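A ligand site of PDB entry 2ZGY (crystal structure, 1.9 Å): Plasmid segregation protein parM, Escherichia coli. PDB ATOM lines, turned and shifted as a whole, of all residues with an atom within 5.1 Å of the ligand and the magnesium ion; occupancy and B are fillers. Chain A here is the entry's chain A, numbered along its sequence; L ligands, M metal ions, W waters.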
ATOM      1  N   ASP A   6     -26.614 -20.786 -20.310  1.00  0.00           N
ATOM      2  CA  ASP A   6     -27.055 -22.162 -20.248  1.00  0.00           C
ATOM      3  C   ASP A   6     -28.519 -21.958 -19.876  1.00  0.00           C
ATOM      4  O   ASP A   6     -28.842 -21.817 -18.689  1.00  0.00           O
ATOM      5  CB  ASP A   6     -26.276 -22.863 -19.138  1.00  0.00           C
ATOM      6  CG  ASP A   6     -26.835 -24.226 -18.817  1.00  0.00           C
ATOM      7  OD1 ASP A   6     -27.714 -24.697 -19.589  1.00  0.00           O
ATOM      8  OD2 ASP A   6     -26.371 -24.810 -17.811  1.00  0.00           O
ATOM      9  N   GLY A   8     -31.422 -23.455 -19.103  1.00  0.00           N
ATOM     10  CA  GLY A   8     -32.070 -24.688 -18.686  1.00  0.00           C
ATOM     11  C   GLY A   8     -33.548 -24.403 -18.418  1.00  0.00           C
ATOM     12  O   GLY A   8     -33.917 -23.262 -18.227  1.00  0.00           O
ATOM     13  N   SER A   9     -34.386 -25.438 -18.356  1.00  0.00           N
ATOM     14  CA  SER A   9     -35.803 -25.157 -18.154  1.00  0.00           C
ATOM     15  C   SER A   9     -36.138 -24.930 -16.684  1.00  0.00           C
ATOM     16  O   SER A   9     -37.276 -24.643 -16.369  1.00  0.00           O
ATOM     17  CB  SER A   9     -36.682 -26.263 -18.755  1.00  0.00           C
ATOM     18  OG  SER A   9     -36.421 -27.471 -18.085  1.00  0.00           O
ATOM     19  N   THR A  10     -35.175 -25.056 -15.778  1.00  0.00           N
ATOM     20  CA  THR A  10     -35.455 -24.760 -14.392  1.00  0.00           C
ATOM     21  C   THR A  10     -34.793 -23.411 -14.089  1.00  0.00           C
ATOM     22  O   THR A  10     -35.458 -22.490 -13.632  1.00  0.00           O
ATOM     23  CB  THR A  10     -34.956 -25.870 -13.418  1.00  0.00           C
ATOM     24  OG1 THR A  10     -35.737 -27.056 -13.620  1.00  0.00           O
ATOM     25  CG2 THR A  10     -35.079 -25.420 -11.967  1.00  0.00           C
ATOM     26  N   ASN A  11     -33.494 -23.287 -14.375  1.00  0.00           N
ATOM     27  CA  ASN A  11     -32.807 -22.008 -14.163  1.00  0.00           C
ATOM     28  C   ASN A  11     -31.959 -21.626 -15.386  1.00  0.00           C
ATOM     29  O   ASN A  11     -31.362 -22.498 -16.016  1.00  0.00           O
ATOM     30  CB  ASN A  11     -31.876 -22.072 -12.981  1.00  0.00           C
ATOM     31  CG  ASN A  11     -32.601 -22.017 -11.665  1.00  0.00           C
ATOM     32  OD1 ASN A  11     -33.585 -21.279 -11.529  1.00  0.00           O
ATOM     33  ND2 ASN A  11     -32.130 -22.765 -10.677  1.00  0.00           N
ATOM     34  N   LYS A  13     -28.608 -19.966 -16.458  1.00  0.00           N
ATOM     35  CA  LYS A  13     -27.337 -19.579 -15.818  1.00  0.00           C
ATOM     36  C   LYS A  13     -26.558 -18.704 -16.813  1.00  0.00           C
ATOM     37  O   LYS A  13     -26.460 -19.059 -17.994  1.00  0.00           O
ATOM     38  CB  LYS A  13     -26.461 -20.803 -15.451  1.00  0.00           C
ATOM     39  CG  LYS A  13     -26.910 -21.555 -14.197  1.00  0.00           C
ATOM     40  CD  LYS A  13     -28.194 -22.381 -14.439  1.00  0.00           C
ATOM     41  CE  LYS A  13     -28.027 -23.536 -15.492  1.00  0.00           C
ATOM     42  NZ  LYS A  13     -29.272 -24.399 -15.558  1.00  0.00           N
ATOM     43  N   GLU A 148     -25.286 -29.304 -24.470  1.00  0.00           N
ATOM     44  CA  GLU A 148     -25.028 -29.393 -23.056  1.00  0.00           C
ATOM     45  C   GLU A 148     -23.991 -30.505 -22.886  1.00  0.00           C
ATOM     46  O   GLU A 148     -23.628 -31.173 -23.863  1.00  0.00           O
ATOM     47  CB  GLU A 148     -26.317 -29.800 -22.315  1.00  0.00           C
ATOM     48  CG  GLU A 148     -27.377 -28.721 -22.494  1.00  0.00           C
ATOM     49  CD  GLU A 148     -28.587 -28.924 -21.604  1.00  0.00           C
ATOM     50  OE1 GLU A 148     -28.833 -30.070 -21.139  1.00  0.00           O
ATOM     51  OE2 GLU A 148     -29.309 -27.924 -21.398  1.00  0.00           O
ATOM     52  N   ASP A 170     -24.990 -35.537 -15.812  1.00  0.00           N
ATOM     53  CA  ASP A 170     -25.654 -34.254 -15.541  1.00  0.00           C
ATOM     54  C   ASP A 170     -27.043 -34.433 -14.920  1.00  0.00           C
ATOM     55  O   ASP A 170     -27.963 -34.870 -15.608  1.00  0.00           O
ATOM     56  CB  ASP A 170     -25.806 -33.499 -16.874  1.00  0.00           C
ATOM     57  CG  ASP A 170     -26.639 -32.227 -16.757  1.00  0.00           C
ATOM     58  OD1 ASP A 170     -26.493 -31.530 -15.725  1.00  0.00           O
ATOM     59  OD2 ASP A 170     -27.415 -31.910 -17.692  1.00  0.00           O
ATOM     60  N   LEU A 171     -27.210 -34.077 -13.644  1.00  0.00           N
ATOM     61  CA  LEU A 171     -28.569 -34.199 -13.042  1.00  0.00           C
ATOM     62  C   LEU A 171     -29.118 -32.776 -12.960  1.00  0.00           C
ATOM     63  O   LEU A 171     -28.589 -31.932 -12.225  1.00  0.00           O
ATOM     64  CB  LEU A 171     -28.484 -34.794 -11.646  1.00  0.00           C
ATOM     65  CG  LEU A 171     -29.841 -34.879 -10.896  1.00  0.00           C
ATOM     66  CD1 LEU A 171     -30.880 -35.620 -11.751  1.00  0.00           C
ATOM     67  CD2 LEU A 171     -29.615 -35.620  -9.561  1.00  0.00           C
ATOM     68  N   GLY A 172     -30.125 -32.503 -13.786  1.00  0.00           N
ATOM     69  CA  GLY A 172     -30.735 -31.191 -13.800  1.00  0.00           C
ATOM     70  C   GLY A 172     -32.056 -31.154 -13.012  1.00  0.00           C
ATOM     71  O   GLY A 172     -32.371 -32.086 -12.293  1.00  0.00           O
ATOM     72  N   GLY A 173     -32.801 -30.067 -13.172  1.00  0.00           N
ATOM     73  CA  GLY A 173     -34.063 -29.929 -12.475  1.00  0.00           C
ATOM     74  C   GLY A 173     -35.110 -30.945 -12.879  1.00  0.00           C
ATOM     75  O   GLY A 173     -35.874 -31.383 -12.031  1.00  0.00           O
ATOM     76  N   THR A 174     -35.146 -31.340 -14.143  1.00  0.00           N
ATOM     77  CA  THR A 174     -36.156 -32.269 -14.573  1.00  0.00           C
ATOM     78  C   THR A 174     -35.649 -33.434 -15.382  1.00  0.00           C
ATOM     79  O   THR A 174     -36.438 -34.298 -15.766  1.00  0.00           O
ATOM     80  CB  THR A 174     -37.257 -31.578 -15.423  1.00  0.00           C
ATOM     81  OG1 THR A 174     -36.651 -30.997 -16.579  1.00  0.00           O
ATOM     82  CG2 THR A 174     -37.953 -30.486 -14.630  1.00  0.00           C
ATOM     83  N   VAL A 199     -33.962 -33.229 -10.182  1.00  0.00           N
ATOM     84  CA  VAL A 199     -33.900 -32.766  -8.813  1.00  0.00           C
ATOM     85  C   VAL A 199     -35.307 -32.435  -8.302  1.00  0.00           C
ATOM     86  O   VAL A 199     -35.580 -32.547  -7.106  1.00  0.00           O
ATOM     87  CB  VAL A 199     -33.049 -31.499  -8.732  1.00  0.00           C
ATOM     88  CG1 VAL A 199     -33.182 -30.868  -7.356  1.00  0.00           C
ATOM     89  CG2 VAL A 199     -31.585 -31.820  -9.006  1.00  0.00           C
ATOM     90  N   ASP A 223     -35.043 -26.040  -1.298  1.00  0.00           N
ATOM     91  CA  ASP A 223     -33.663 -26.261  -1.685  1.00  0.00           C
ATOM     92  C   ASP A 223     -32.740 -26.183  -0.476  1.00  0.00           C
ATOM     93  O   ASP A 223     -31.804 -26.966  -0.378  1.00  0.00           O
ATOM     94  CB  ASP A 223     -33.203 -25.270  -2.765  1.00  0.00           C
ATOM     95  CG  ASP A 223     -33.888 -25.499  -4.112  1.00  0.00           C
ATOM     96  OD1 ASP A 223     -33.932 -26.660  -4.580  1.00  0.00           O
ATOM     97  OD2 ASP A 223     -34.356 -24.494  -4.698  1.00  0.00           O
ATOM     98  N   ILE A 226     -32.728 -29.291   1.500  1.00  0.00           N
ATOM     99  CA  ILE A 226     -31.983 -30.322   0.799  1.00  0.00           C
ATOM    100  C   ILE A 226     -30.499 -30.130   0.925  1.00  0.00           C
ATOM    101  O   ILE A 226     -29.762 -31.052   1.281  1.00  0.00           O
ATOM    102  CB  ILE A 226     -32.390 -30.355  -0.697  1.00  0.00           C
ATOM    103  CG1 ILE A 226     -33.844 -30.860  -0.802  1.00  0.00           C
ATOM    104  CG2 ILE A 226     -31.456 -31.305  -1.495  1.00  0.00           C
ATOM    105  CD1 ILE A 226     -34.438 -30.808  -2.211  1.00  0.00           C
ATOM    106  N   ILE A 227     -30.047 -28.930   0.596  1.00  0.00           N
ATOM    107  CA  ILE A 227     -28.645 -28.591   0.645  1.00  0.00           C
ATOM    108  C   ILE A 227     -28.096 -28.829   2.030  1.00  0.00           C
ATOM    109  O   ILE A 227     -26.984 -29.316   2.154  1.00  0.00           O
ATOM    110  CB  ILE A 227     -28.430 -27.120   0.273  1.00  0.00           C
ATOM    111  CG1 ILE A 227     -28.640 -26.949  -1.226  1.00  0.00           C
ATOM    112  CG2 ILE A 227     -27.051 -26.656   0.720  1.00  0.00           C
ATOM    113  CD1 ILE A 227     -28.980 -25.521  -1.593  1.00  0.00           C
ATOM    114  N   ARG A 229     -29.369 -30.903   4.301  1.00  0.00           N
ATOM    115  CA  ARG A 229     -29.982 -32.117   4.834  1.00  0.00           C
ATOM    116  C   ARG A 229     -29.099 -32.844   5.848  1.00  0.00           C
ATOM    117  O   ARG A 229     -29.604 -33.585   6.680  1.00  0.00           O
ATOM    118  CB  ARG A 229     -30.387 -33.056   3.671  1.00  0.00           C
ATOM    119  CG  ARG A 229     -29.222 -33.505   2.791  1.00  0.00           C
ATOM    120  CD  ARG A 229     -29.676 -34.402   1.627  1.00  0.00           C
ATOM    121  NE  ARG A 229     -28.525 -34.940   0.905  1.00  0.00           N
ATOM    122  CZ  ARG A 229     -27.691 -34.229   0.146  1.00  0.00           C
ATOM    123  NH1 ARG A 229     -26.675 -34.842  -0.453  1.00  0.00           N
ATOM    124  NH2 ARG A 229     -27.890 -32.922  -0.063  1.00  0.00           N
ATOM    125  N   GLY A 280     -24.246 -30.390 -13.049  1.00  0.00           N
ATOM    126  CA  GLY A 280     -25.632 -29.979 -12.913  1.00  0.00           C
ATOM    127  C   GLY A 280     -25.957 -29.629 -11.475  1.00  0.00           C
ATOM    128  O   GLY A 280     -25.194 -29.982 -10.556  1.00  0.00           O
ATOM    129  N   GLY A 281     -27.102 -29.002 -11.267  1.00  0.00           N
ATOM    130  CA  GLY A 281     -27.514 -28.630  -9.935  1.00  0.00           C
ATOM    131  C   GLY A 281     -27.661 -29.813  -9.006  1.00  0.00           C
ATOM    132  O   GLY A 281     -27.466 -29.686  -7.785  1.00  0.00           O
ATOM    133  N   GLY A 282     -28.018 -30.975  -9.533  1.00  0.00           N
ATOM    134  CA  GLY A 282     -28.156 -32.080  -8.627  1.00  0.00           C
ATOM    135  C   GLY A 282     -26.926 -32.936  -8.438  1.00  0.00           C
ATOM    136  O   GLY A 282     -27.018 -34.010  -7.872  1.00  0.00           O
ATOM    137  N   GLU A 284     -24.375 -32.989  -6.319  1.00  0.00           N
ATOM    138  CA  GLU A 284     -24.053 -33.403  -4.948  1.00  0.00           C
ATOM    139  C   GLU A 284     -25.014 -34.475  -4.393  1.00  0.00           C
ATOM    140  O   GLU A 284     -24.684 -35.172  -3.422  1.00  0.00           O
ATOM    141  CB  GLU A 284     -24.055 -32.176  -4.010  1.00  0.00           C
ATOM    142  CG  GLU A 284     -25.400 -31.470  -3.897  1.00  0.00           C
ATOM    143  CD  GLU A 284     -25.953 -31.403  -2.437  1.00  0.00           C
ATOM    144  OE1 GLU A 284     -26.743 -30.468  -2.130  1.00  0.00           O
ATOM    145  OE2 GLU A 284     -25.604 -32.289  -1.618  1.00  0.00           O
ATOM    146  N   LEU A 285     -26.156 -34.617  -5.043  1.00  0.00           N
ATOM    147  CA  LEU A 285     -27.178 -35.574  -4.613  1.00  0.00           C
ATOM    148  C   LEU A 285     -26.878 -36.982  -5.059  1.00  0.00           C
ATOM    149  O   LEU A 285     -27.392 -37.942  -4.451  1.00  0.00           O
ATOM    150  CB  LEU A 285     -28.561 -35.159  -5.175  1.00  0.00           C
ATOM    151  CG  LEU A 285     -29.012 -33.732  -4.855  1.00  0.00           C
ATOM    152  CD1 LEU A 285     -30.425 -33.505  -5.332  1.00  0.00           C
ATOM    153  CD2 LEU A 285     -28.952 -33.512  -3.344  1.00  0.00           C
ATOM    154  N   GLN A 308     -23.964 -26.314 -10.598  1.00  0.00           N
ATOM    155  CA  GLN A 308     -24.997 -25.780 -11.468  1.00  0.00           C
ATOM    156  C   GLN A 308     -24.412 -24.879 -12.581  1.00  0.00           C
ATOM    157  O   GLN A 308     -25.068 -24.641 -13.600  1.00  0.00           O
ATOM    158  CB  GLN A 308     -26.025 -24.988 -10.675  1.00  0.00           C
ATOM    159  CG  GLN A 308     -25.510 -23.703 -10.096  1.00  0.00           C
ATOM    160  CD  GLN A 308     -26.520 -23.098  -9.100  1.00  0.00           C
ATOM    161  OE1 GLN A 308     -27.748 -23.247  -9.265  1.00  0.00           O
ATOM    162  NE2 GLN A 308     -25.996 -22.401  -8.084  1.00  0.00           N
HETATM  163  P1  LIG L   1     -31.660 -26.899 -15.291  1.00  0.00           P
HETATM  164  O1  LIG L   1     -30.459 -26.892 -16.102  1.00  0.00           O
HETATM  165  O2  LIG L   1     -32.234 -25.548 -15.418  1.00  0.00           O
HETATM  166  O3  LIG L   1     -32.436 -28.175 -15.675  1.00  0.00           O
HETATM  167  O4  LIG L   1     -30.774 -27.351 -14.104  1.00  0.00           O
HETATM  168  P2  LIG L   1     -29.973 -27.022 -12.852  1.00  0.00           P
HETATM  169  O5  LIG L   1     -29.262 -25.721 -12.997  1.00  0.00           O
HETATM  170  O6  LIG L   1     -29.158 -28.244 -12.899  1.00  0.00           O
HETATM  171  O7  LIG L   1     -30.811 -27.007 -11.477  1.00  0.00           O
HETATM  172  C1  LIG L   1     -31.199 -28.207 -10.869  1.00  0.00           C
HETATM  173  C2  LIG L   1     -31.793 -27.901  -9.479  1.00  0.00           C
HETATM  174  O8  LIG L   1     -30.735 -28.079  -8.507  1.00  0.00           O
HETATM  175  C3  LIG L   1     -32.339 -26.478  -9.280  1.00  0.00           C
HETATM  176  O9  LIG L   1     -33.627 -26.476  -8.682  1.00  0.00           O
HETATM  177  C4  LIG L   1     -31.286 -25.749  -8.454  1.00  0.00           C
HETATM  178  O10 LIG L   1     -31.728 -24.685  -7.600  1.00  0.00           O
HETATM  179  C5  LIG L   1     -30.694 -26.908  -7.664  1.00  0.00           C
HETATM  180  N1  LIG L   1     -29.312 -26.723  -7.202  1.00  0.00           N
HETATM  181  C6  LIG L   1     -28.310 -25.910  -7.636  1.00  0.00           C
HETATM  182  N2  LIG L   1     -27.189 -26.019  -7.007  1.00  0.00           N
HETATM  183  C7  LIG L   1     -27.458 -26.999  -6.069  1.00  0.00           C
HETATM  184  C8  LIG L   1     -26.609 -27.580  -5.056  1.00  0.00           C
HETATM  185  O11 LIG L   1     -25.417 -27.297  -4.821  1.00  0.00           O
HETATM  186  N3  LIG L   1     -27.270 -28.581  -4.306  1.00  0.00           N
HETATM  187  C9  LIG L   1     -28.596 -28.973  -4.482  1.00  0.00           C
HETATM  188  N4  LIG L   1     -29.049 -29.930  -3.669  1.00  0.00           N
HETATM  189  N5  LIG L   1     -29.405 -28.411  -5.422  1.00  0.00           N
HETATM  190  C10 LIG L   1     -28.755 -27.437  -6.177  1.00  0.00           C
HETATM  191 MG    MG M   1     -29.116 -28.074 -17.234  1.00  0.00          MG
HETATM  192  O   HOH W   1     -34.954 -28.464 -15.792  1.00  0.00           O
HETATM  193  O   HOH W   2     -28.619 -29.370 -15.583  1.00  0.00           O
HETATM  194  O   HOH W   3     -30.954 -29.179 -17.632  1.00  0.00           O
HETATM  195  O   HOH W   4     -27.215 -27.167 -16.736  1.00  0.00           O
HETATM  196  O   HOH W   5     -26.771 -26.706 -14.225  1.00  0.00           O
HETATM  197  O   HOH W   6     -33.134 -30.875 -16.204  1.00  0.00           O
HETATM  198  O   HOH W   7     -24.978 -30.059  -6.913  1.00  0.00           O
HETATM  199  O   HOH W   8     -28.211 -29.587 -18.492  1.00  0.00           O
HETATM  200  O   HOH W   9     -22.640 -27.830  -6.168  1.00  0.00           O
HETATM  201  O   HOH W  10     -29.454 -26.800 -18.882  1.00  0.00           O
HETATM  202  O   HOH W  11     -31.844 -29.148  -4.335  1.00  0.00           O
HETATM  203  O   HOH W  12     -29.865 -22.744  -7.635  1.00  0.00           O
HETATM  204  O   HOH W  13     -24.378 -25.786  -7.809  1.00  0.00           O
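The magnesium ion is bound by water W10 (2.1 Å). O1 of the ligand binds the magnesium ion (2.1 Å). Water W2 is bound to the magnesium ion. Water W4 is bound to the magnesium ion (2.2 Å). Water W8 is bound to the magnesium ion (2.2 Å). Water W3 binds the magnesium ion (2.2 Å). The magnesium ion has six donor atoms within binding distance.
An oxygen (O6) of the ligand sits at hydrogen-bond distance from the backbone NH of Gly 281 (2.7 Å). N of Asn 11 sits at hydrogen-bond distance from O2 of the ligand. O3 of the ligand lies within hydrogen-bond range of N of Gly 173, 3.2 Å away. N of Thr 10 is in hydrogen-bond range of O2 of the ligand, 3.0 Å away. The side-chain carboxylate (OE1) of Glu 284 is in hydrogen-bond range of a nitrogen (N4) of the ligand, at 2.8 Å. An oxygen (O5) of the ligand is in salt-bridge range of the side-chain amino group (NZ) of Lys 13.
CA of Gly 8 touches O2 of the ligand (3.4 Å). Ser 9 touches the ligand (N to O2, 3.6 Å). O of Leu 171 touches O6 of the ligand, 3.8 Å away. CA of Gly 172 touches O6 of the ligand (3.5 Å). Val 199 touches the ligand. Asp 223 touches the ligand (OD2 to O10, 3.9 Å). CG2 of Ile 226 touches N4 of the ligand, at 3.5 Å. CG1 of Ile 227 touches N3 of the ligand (3.7 Å). Gly 280 touches the ligand. CD2 of Leu 285 touches N4 of the ligand, 3.6 Å away. Gln 308 touches the ligand. 17 residues have an atom within 4 Å of the ligand: Gly 8, Ser 9, Thr 10, Asn 11, Lys 13, Leu 171, Gly 172, Gly 173, Val 199, Asp 223, Ile 226, Ile 227, Gly 280, Gly 281, Glu 284, Leu 285 and Gln 308.
No residue comes within 4 Å of the magnesium ion.
The side-chain amino group (NZ) of Lys 13 is in salt-bridge range of the side-chain carboxylate (OD2) of Asp 6 (3.7 Å). The backbone carbonyl oxygen of Ile 226 sits close to the guanidinium group of Arg 229 (3.0 Å). The backbone NH (N) of Val 199 sits at hydrogen-bond distance from the backbone carbonyl oxygen (O) of Gly 172, 2.9 Å away. The guanidinium group of Arg 229 is in salt-bridge range of the side-chain carboxylate of Glu 284 (2.8 Å). O of Gly 173 sits at hydrogen-bond distance from N of Val 199 (3.2 Å). The backbone carbonyl oxygen (O) of Leu 171 sits at hydrogen-bond distance from the backbone NH (N) of Gly 282. N of Gly 281 sits at hydrogen-bond distance from O of Leu 171, 3.4 Å away. O of Asn 11 is in hydrogen-bond range of NZ of Lys 13, 2.9 Å away.
Water W2 lies within hydrogen-bond range of O6 of the ligand (3.0 Å) and OD1 of Asp 170 (3.0 Å). Water W1 lies within hydrogen-bond range of an oxygen (O3) of the ligand, the side-chain hydroxyl (OG1) of Thr 10, the side-chain hydroxyl (OG) of Ser 9 and the side-chain hydroxyl (OG1) of Thr 174. Water W6 lies within hydrogen-bond range of an oxygen (O3) of the ligand (2.8 Å), the backbone NH (N) of Thr 174 (2.9 Å) and the backbone NH (N) of Gly 173 (3.2 Å). Water W13 bridges the backbone NH (N) of Gln 308 and a nitrogen (N2) of the ligand. Water W5 bridges O of Gln 308 and O5 of the ligand. Water W7 lies within hydrogen-bond range of the backbone carbonyl oxygen (O) of Gly 281 (2.7 Å), the backbone NH (N) of Glu 284 (3.0 Å) and an oxygen (O11) of the ligand (3.5 Å).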
